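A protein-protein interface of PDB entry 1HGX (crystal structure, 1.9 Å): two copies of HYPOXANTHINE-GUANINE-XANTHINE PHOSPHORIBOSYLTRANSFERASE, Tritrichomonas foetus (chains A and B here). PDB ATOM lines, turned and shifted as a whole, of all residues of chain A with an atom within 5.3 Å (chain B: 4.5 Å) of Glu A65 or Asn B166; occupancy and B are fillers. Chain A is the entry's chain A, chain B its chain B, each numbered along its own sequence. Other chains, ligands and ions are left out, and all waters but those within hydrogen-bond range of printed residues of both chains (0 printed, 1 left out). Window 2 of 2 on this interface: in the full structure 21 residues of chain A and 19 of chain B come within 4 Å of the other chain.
O of Leu A64 lies within hydrogen-bond range of NH2 of Arg B169. The side-chain amide nitrogen of Gln A63 lies within hydrogen-bond range of the backbone carbonyl oxygen of His B165, 2.8 Å away. The backbone NH (N) of Leu A64 lies within hydrogen-bond range of the backbone carbonyl oxygen (O) of Asn B166.
Met A42 touches none of the printed residues of chain B. Of the printed residues of chain B, Gln A63 touches His B165, Asn B166 and Lys B167. Of the printed residues of chain B, Leu A64 touches Asn B166 (3.1 Å) and Arg B169 (2.6 Å). Of the printed residues of chain B, Glu A65 touches Asn B166 (3.9 Å). Arg A96 touches none of the printed residues of chain B. Of the printed residues of chain A, His B165 touches Gln A63 (2.8 Å). Asn B166 touches just these residues of chain A: Gln A63 (3.4 Å), Leu A64 (3.1 Å) and Glu A65 (3.9 Å). Of the printed residues of chain A, Lys B167 touches Gln A63. Printed residues of chain A within 4 Å of Arg B169: Leu A64 (2.6 Å) and Pro A66 (3.5 Å). The nearest printed residue of chain A that does not touch Asn B166 is Pro A66 (4.2 Å). The nearest printed residue of chain A that does not touch Arg B169 is Glu A65 (4.6 Å).
Among the printed residues, pairs that only touch across the chains: Gln A63 with Asn B166, Pro A66 with Arg B169, Glu A65 with Asn B166 and Gln A63 with Lys B167.
N of Met A42 is in hydrogen-bond range of O of Glu A65. O of Pro A40 lies within hydrogen-bond range of N of Glu A65. The side-chain carboxylate (OD2) of Asp B163 lies within salt-bridge range of the guanidinium group (NH1) of Arg B169. OD1 of Asn B166 is in hydrogen-bond range of NH1 of Arg B169 (3.1 Å). OE1 of Glu A65 lies within salt-bridge range of NH2 of Arg A96 (2.9 Å). N of Asn B166 lies within hydrogen-bond range of OD2 of Asp B163, 2.9 Å away.
Printed residues of chain A that touch a printed residue of chain B: Gln A63, Leu A64, Glu A65 and Pro A66. Hydrophobic or aromatic side chains of chain A within 4 Å of the printed part of chain B: Leu A64 and Pro A66.
No position is printed for both chains.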
ATOM      1  N   ASN A  39      -6.898  28.563  36.768  1.00  0.00           N
ATOM      2  CA  ASN A  39      -6.149  27.719  35.825  1.00  0.00           C
ATOM      3  C   ASN A  39      -6.719  26.302  35.867  1.00  0.00           C
ATOM      4  O   ASN A  39      -6.011  25.332  36.151  1.00  0.00           O
ATOM      5  CB  ASN A  39      -4.660  27.685  36.178  1.00  0.00           C
ATOM      6  CG  ASN A  39      -3.843  26.934  35.148  1.00  0.00           C
ATOM      7  OD1 ASN A  39      -2.821  26.333  35.468  1.00  0.00           O
ATOM      8  ND2 ASN A  39      -4.303  26.949  33.900  1.00  0.00           N
ATOM      9  N   PRO A  40      -8.022  26.166  35.565  1.00  0.00           N
ATOM     10  CA  PRO A  40      -8.677  24.861  35.591  1.00  0.00           C
ATOM     11  C   PRO A  40      -8.401  23.937  34.430  1.00  0.00           C
ATOM     12  O   PRO A  40      -7.989  24.365  33.353  1.00  0.00           O
ATOM     13  CB  PRO A  40     -10.155  25.252  35.595  1.00  0.00           C
ATOM     14  CG  PRO A  40     -10.159  26.388  34.600  1.00  0.00           C
ATOM     15  CD  PRO A  40      -8.954  27.205  35.079  1.00  0.00           C
ATOM     16  N   VAL A  41      -8.660  22.655  34.661  1.00  0.00           N
ATOM     17  CA  VAL A  41      -8.546  21.642  33.629  1.00  0.00           C
ATOM     18  C   VAL A  41     -10.007  21.502  33.162  1.00  0.00           C
ATOM     19  O   VAL A  41     -10.890  21.142  33.942  1.00  0.00           O
ATOM     20  CB  VAL A  41      -8.042  20.292  34.189  1.00  0.00           C
ATOM     21  CG1 VAL A  41      -7.990  19.251  33.076  1.00  0.00           C
ATOM     22  CG2 VAL A  41      -6.657  20.461  34.801  1.00  0.00           C
ATOM     23  N   MET A  42     -10.267  21.864  31.916  1.00  0.00           N
ATOM     24  CA  MET A  42     -11.613  21.791  31.353  1.00  0.00           C
ATOM     25  C   MET A  42     -11.677  20.519  30.537  1.00  0.00           C
ATOM     26  O   MET A  42     -11.074  20.429  29.472  1.00  0.00           O
ATOM     27  CB  MET A  42     -11.850  22.971  30.417  1.00  0.00           C
ATOM     28  CG  MET A  42     -11.453  24.292  30.991  1.00  0.00           C
ATOM     29  SD  MET A  42     -12.791  24.966  31.900  1.00  0.00           S
ATOM     30  CE  MET A  42     -13.684  25.566  30.614  1.00  0.00           C
ATOM     31  N   TYR A  53     -18.329  22.601  23.715  1.00  0.00           N
ATOM     32  CA  TYR A  53     -17.031  22.839  24.356  1.00  0.00           C
ATOM     33  C   TYR A  53     -16.209  23.917  23.652  1.00  0.00           C
ATOM     34  O   TYR A  53     -15.761  24.879  24.291  1.00  0.00           O
ATOM     35  CB  TYR A  53     -16.232  21.534  24.411  1.00  0.00           C
ATOM     36  CG  TYR A  53     -14.887  21.619  25.113  1.00  0.00           C
ATOM     37  CD1 TYR A  53     -14.803  21.591  26.506  1.00  0.00           C
ATOM     38  CD2 TYR A  53     -13.694  21.647  24.383  1.00  0.00           C
ATOM     39  CE1 TYR A  53     -13.563  21.577  27.158  1.00  0.00           C
ATOM     40  CE2 TYR A  53     -12.450  21.633  25.028  1.00  0.00           C
ATOM     41  CZ  TYR A  53     -12.394  21.596  26.412  1.00  0.00           C
ATOM     42  OH  TYR A  53     -11.168  21.564  27.049  1.00  0.00           O
ATOM     43  N   PHE A  62      -9.243  33.550  29.735  1.00  0.00           N
ATOM     44  CA  PHE A  62      -8.279  33.304  30.807  1.00  0.00           C
ATOM     45  C   PHE A  62      -7.521  32.000  30.572  1.00  0.00           C
ATOM     46  O   PHE A  62      -7.892  31.204  29.705  1.00  0.00           O
ATOM     47  CB  PHE A  62      -8.953  33.321  32.188  1.00  0.00           C
ATOM     48  CG  PHE A  62     -10.135  32.395  32.317  1.00  0.00           C
ATOM     49  CD1 PHE A  62      -9.962  31.057  32.657  1.00  0.00           C
ATOM     50  CD2 PHE A  62     -11.432  32.876  32.147  1.00  0.00           C
ATOM     51  CE1 PHE A  62     -11.060  30.215  32.828  1.00  0.00           C
ATOM     52  CE2 PHE A  62     -12.544  32.036  32.315  1.00  0.00           C
ATOM     53  CZ  PHE A  62     -12.355  30.704  32.657  1.00  0.00           C
ATOM     54  N   GLN A  63      -6.426  31.811  31.301  1.00  0.00           N
ATOM     55  CA  GLN A  63      -5.614  30.610  31.166  1.00  0.00           C
ATOM     56  C   GLN A  63      -6.377  29.395  31.690  1.00  0.00           C
ATOM     57  O   GLN A  63      -6.913  29.410  32.798  1.00  0.00           O
ATOM     58  CB  GLN A  63      -4.305  30.785  31.932  1.00  0.00           C
ATOM     59  CG  GLN A  63      -3.337  29.637  31.791  1.00  0.00           C
ATOM     60  CD  GLN A  63      -2.054  29.880  32.555  1.00  0.00           C
ATOM     61  OE1 GLN A  63      -2.073  30.352  33.683  1.00  0.00           O
ATOM     62  NE2 GLN A  63      -0.931  29.566  31.938  1.00  0.00           N
ATOM     63  N   LEU A  64      -6.433  28.349  30.876  1.00  0.00           N
ATOM     64  CA  LEU A  64      -7.125  27.109  31.230  1.00  0.00           C
ATOM     65  C   LEU A  64      -6.437  25.987  30.470  1.00  0.00           C
ATOM     66  O   LEU A  64      -5.800  26.229  29.452  1.00  0.00           O
ATOM     67  CB  LEU A  64      -8.606  27.201  30.849  1.00  0.00           C
ATOM     68  CG  LEU A  64      -8.977  27.483  29.390  1.00  0.00           C
ATOM     69  CD1 LEU A  64      -9.112  26.192  28.585  1.00  0.00           C
ATOM     70  CD2 LEU A  64     -10.280  28.258  29.376  1.00  0.00           C
ATOM     71  N   GLU A  65      -6.565  24.760  30.949  1.00  0.00           N
ATOM     72  CA  GLU A  65      -5.910  23.628  30.316  1.00  0.00           C
ATOM     73  C   GLU A  65      -6.934  22.634  29.795  1.00  0.00           C
ATOM     74  O   GLU A  65      -7.652  22.016  30.570  1.00  0.00           O
ATOM     75  CB  GLU A  65      -5.006  22.964  31.343  1.00  0.00           C
ATOM     76  CG  GLU A  65      -4.196  21.799  30.827  1.00  0.00           C
ATOM     77  CD  GLU A  65      -3.017  21.484  31.724  1.00  0.00           C
ATOM     78  OE1 GLU A  65      -2.925  22.061  32.832  1.00  0.00           O
ATOM     79  OE2 GLU A  65      -2.171  20.661  31.314  1.00  0.00           O
ATOM     80  N   PRO A  66      -7.047  22.496  28.473  1.00  0.00           N
ATOM     81  CA  PRO A  66      -8.029  21.548  27.952  1.00  0.00           C
ATOM     82  C   PRO A  66      -7.565  20.104  28.098  1.00  0.00           C
ATOM     83  O   PRO A  66      -6.366  19.824  28.112  1.00  0.00           O
ATOM     84  CB  PRO A  66      -8.117  21.917  26.460  1.00  0.00           C
ATOM     85  CG  PRO A  66      -7.612  23.317  26.390  1.00  0.00           C
ATOM     86  CD  PRO A  66      -6.461  23.283  27.382  1.00  0.00           C
ATOM     87  N   ASP A  67      -8.525  19.200  28.247  1.00  0.00           N
ATOM     88  CA  ASP A  67      -8.238  17.781  28.316  1.00  0.00           C
ATOM     89  C   ASP A  67      -9.479  17.079  27.786  1.00  0.00           C
ATOM     90  O   ASP A  67     -10.560  17.666  27.733  1.00  0.00           O
ATOM     91  CB  ASP A  67      -7.884  17.324  29.725  1.00  0.00           C
ATOM     92  CG  ASP A  67      -6.954  16.109  29.724  1.00  0.00           C
ATOM     93  OD1 ASP A  67      -6.910  15.348  28.727  1.00  0.00           O
ATOM     94  OD2 ASP A  67      -6.252  15.917  30.734  1.00  0.00           O
ATOM     95  N   THR A  91      -3.715  14.897  31.698  1.00  0.00           N
ATOM     96  CA  THR A  91      -3.396  15.705  32.869  1.00  0.00           C
ATOM     97  C   THR A  91      -3.613  15.026  34.215  1.00  0.00           C
ATOM     98  O   THR A  91      -4.594  14.306  34.415  1.00  0.00           O
ATOM     99  CB  THR A  91      -4.248  16.989  32.862  1.00  0.00           C
ATOM    100  OG1 THR A  91      -4.172  17.587  31.563  1.00  0.00           O
ATOM    101  CG2 THR A  91      -3.750  17.982  33.905  1.00  0.00           C
ATOM    102  N   ARG A  96      -5.995  20.155  41.223  1.00  0.00           N
ATOM    103  CA  ARG A  96      -6.420  21.103  40.195  1.00  0.00           C
ATOM    104  C   ARG A  96      -7.919  21.335  40.266  1.00  0.00           C
ATOM    105  O   ARG A  96      -8.651  20.499  40.791  1.00  0.00           O
ATOM    106  CB  ARG A  96      -6.094  20.547  38.813  1.00  0.00           C
ATOM    107  CG  ARG A  96      -4.614  20.286  38.566  1.00  0.00           C
ATOM    108  CD  ARG A  96      -3.846  21.580  38.385  1.00  0.00           C
ATOM    109  NE  ARG A  96      -4.364  22.376  37.274  1.00  0.00           N
ATOM    110  CZ  ARG A  96      -3.968  22.266  36.008  1.00  0.00           C
ATOM    111  NH1 ARG A  96      -3.047  21.374  35.677  1.00  0.00           N
ATOM    112  NH2 ARG A  96      -4.462  23.084  35.077  1.00  0.00           N
ATOM    113  N   ASP B 163      -2.300  28.447  21.060  1.00  0.00           N
ATOM    114  CA  ASP B 163      -2.054  29.046  22.358  1.00  0.00           C
ATOM    115  C   ASP B 163      -0.582  29.250  22.680  1.00  0.00           C
ATOM    116  O   ASP B 163       0.302  28.770  21.977  1.00  0.00           O
ATOM    117  CB  ASP B 163      -2.633  28.134  23.448  1.00  0.00           C
ATOM    118  CG  ASP B 163      -1.757  26.904  23.705  1.00  0.00           C
ATOM    119  OD1 ASP B 163      -1.688  26.021  22.827  1.00  0.00           O
ATOM    120  OD2 ASP B 163      -1.085  26.849  24.758  1.00  0.00           O
ATOM    121  N   PHE B 164      -0.348  29.990  23.757  1.00  0.00           N
ATOM    122  CA  PHE B 164       0.983  30.195  24.298  1.00  0.00           C
ATOM    123  C   PHE B 164       0.716  30.127  25.791  1.00  0.00           C
ATOM    124  O   PHE B 164      -0.044  30.932  26.326  1.00  0.00           O
ATOM    125  CB  PHE B 164       1.605  31.544  23.957  1.00  0.00           C
ATOM    126  CG  PHE B 164       2.916  31.772  24.666  1.00  0.00           C
ATOM    127  CD1 PHE B 164       4.043  31.038  24.315  1.00  0.00           C
ATOM    128  CD2 PHE B 164       2.997  32.640  25.748  1.00  0.00           C
ATOM    129  CE1 PHE B 164       5.223  31.152  25.030  1.00  0.00           C
ATOM    130  CE2 PHE B 164       4.180  32.764  26.475  1.00  0.00           C
ATOM    131  CZ  PHE B 164       5.291  32.017  26.115  1.00  0.00           C
ATOM    132  N   HIS B 165       1.287  29.122  26.444  1.00  0.00           N
ATOM    133  CA  HIS B 165       1.095  28.921  27.875  1.00  0.00           C
ATOM    134  C   HIS B 165      -0.391  28.867  28.218  1.00  0.00           C
ATOM    135  O   HIS B 165      -0.843  29.506  29.163  1.00  0.00           O
ATOM    136  CB  HIS B 165       1.794  30.017  28.680  1.00  0.00           C
ATOM    137  CG  HIS B 165       3.284  29.887  28.711  1.00  0.00           C
ATOM    138  ND1 HIS B 165       4.098  30.772  29.381  1.00  0.00           N
ATOM    139  CD2 HIS B 165       4.107  28.970  28.148  1.00  0.00           C
ATOM    140  CE1 HIS B 165       5.358  30.413  29.232  1.00  0.00           C
ATOM    141  NE2 HIS B 165       5.391  29.318  28.483  1.00  0.00           N
ATOM    142  N   ASN B 166      -1.140  28.105  27.425  1.00  0.00           N
ATOM    143  CA  ASN B 166      -2.578  27.938  27.633  1.00  0.00           C
ATOM    144  C   ASN B 166      -3.356  29.240  27.635  1.00  0.00           C
ATOM    145  O   ASN B 166      -4.386  29.360  28.304  1.00  0.00           O
ATOM    146  CB  ASN B 166      -2.844  27.164  28.922  1.00  0.00           C
ATOM    147  CG  ASN B 166      -2.545  25.688  28.777  1.00  0.00           C
ATOM    148  OD1 ASN B 166      -2.712  25.109  27.701  1.00  0.00           O
ATOM    149  ND2 ASN B 166      -2.086  25.073  29.854  1.00  0.00           N
ATOM    150  N   LYS B 167      -2.854  30.215  26.884  1.00  0.00           N
ATOM    151  CA  LYS B 167      -3.494  31.518  26.760  1.00  0.00           C
ATOM    152  C   LYS B 167      -3.645  31.810  25.272  1.00  0.00           C
ATOM    153  O   LYS B 167      -2.993  31.164  24.451  1.00  0.00           O
ATOM    154  CB  LYS B 167      -2.618  32.606  27.407  1.00  0.00           C
ATOM    155  CG  LYS B 167      -2.784  32.743  28.912  1.00  0.00           C
ATOM    156  CD  LYS B 167      -1.457  33.015  29.624  1.00  0.00           C
ATOM    157  CE  LYS B 167      -0.784  34.308  29.180  1.00  0.00           C
ATOM    158  NZ  LYS B 167      -1.482  35.550  29.629  1.00  0.00           N
ATOM    159  N   ARG B 169      -5.972  31.139  22.981  1.00  0.00           N
ATOM    160  CA  ARG B 169      -6.825  30.270  22.153  1.00  0.00           C
ATOM    161  C   ARG B 169      -8.169  30.894  21.766  1.00  0.00           C
ATOM    162  O   ARG B 169      -8.733  30.568  20.721  1.00  0.00           O
ATOM    163  CB  ARG B 169      -7.119  28.958  22.881  1.00  0.00           C
ATOM    164  CG  ARG B 169      -6.098  27.878  22.658  1.00  0.00           C
ATOM    165  CD  ARG B 169      -6.495  26.613  23.399  1.00  0.00           C
ATOM    166  NE  ARG B 169      -6.486  26.841  24.834  1.00  0.00           N
ATOM    167  CZ  ARG B 169      -5.589  26.333  25.673  1.00  0.00           C
ATOM    168  NH1 ARG B 169      -4.617  25.536  25.246  1.00  0.00           N
ATOM    169  NH2 ARG B 169      -5.623  26.700  26.939  1.00  0.00           N
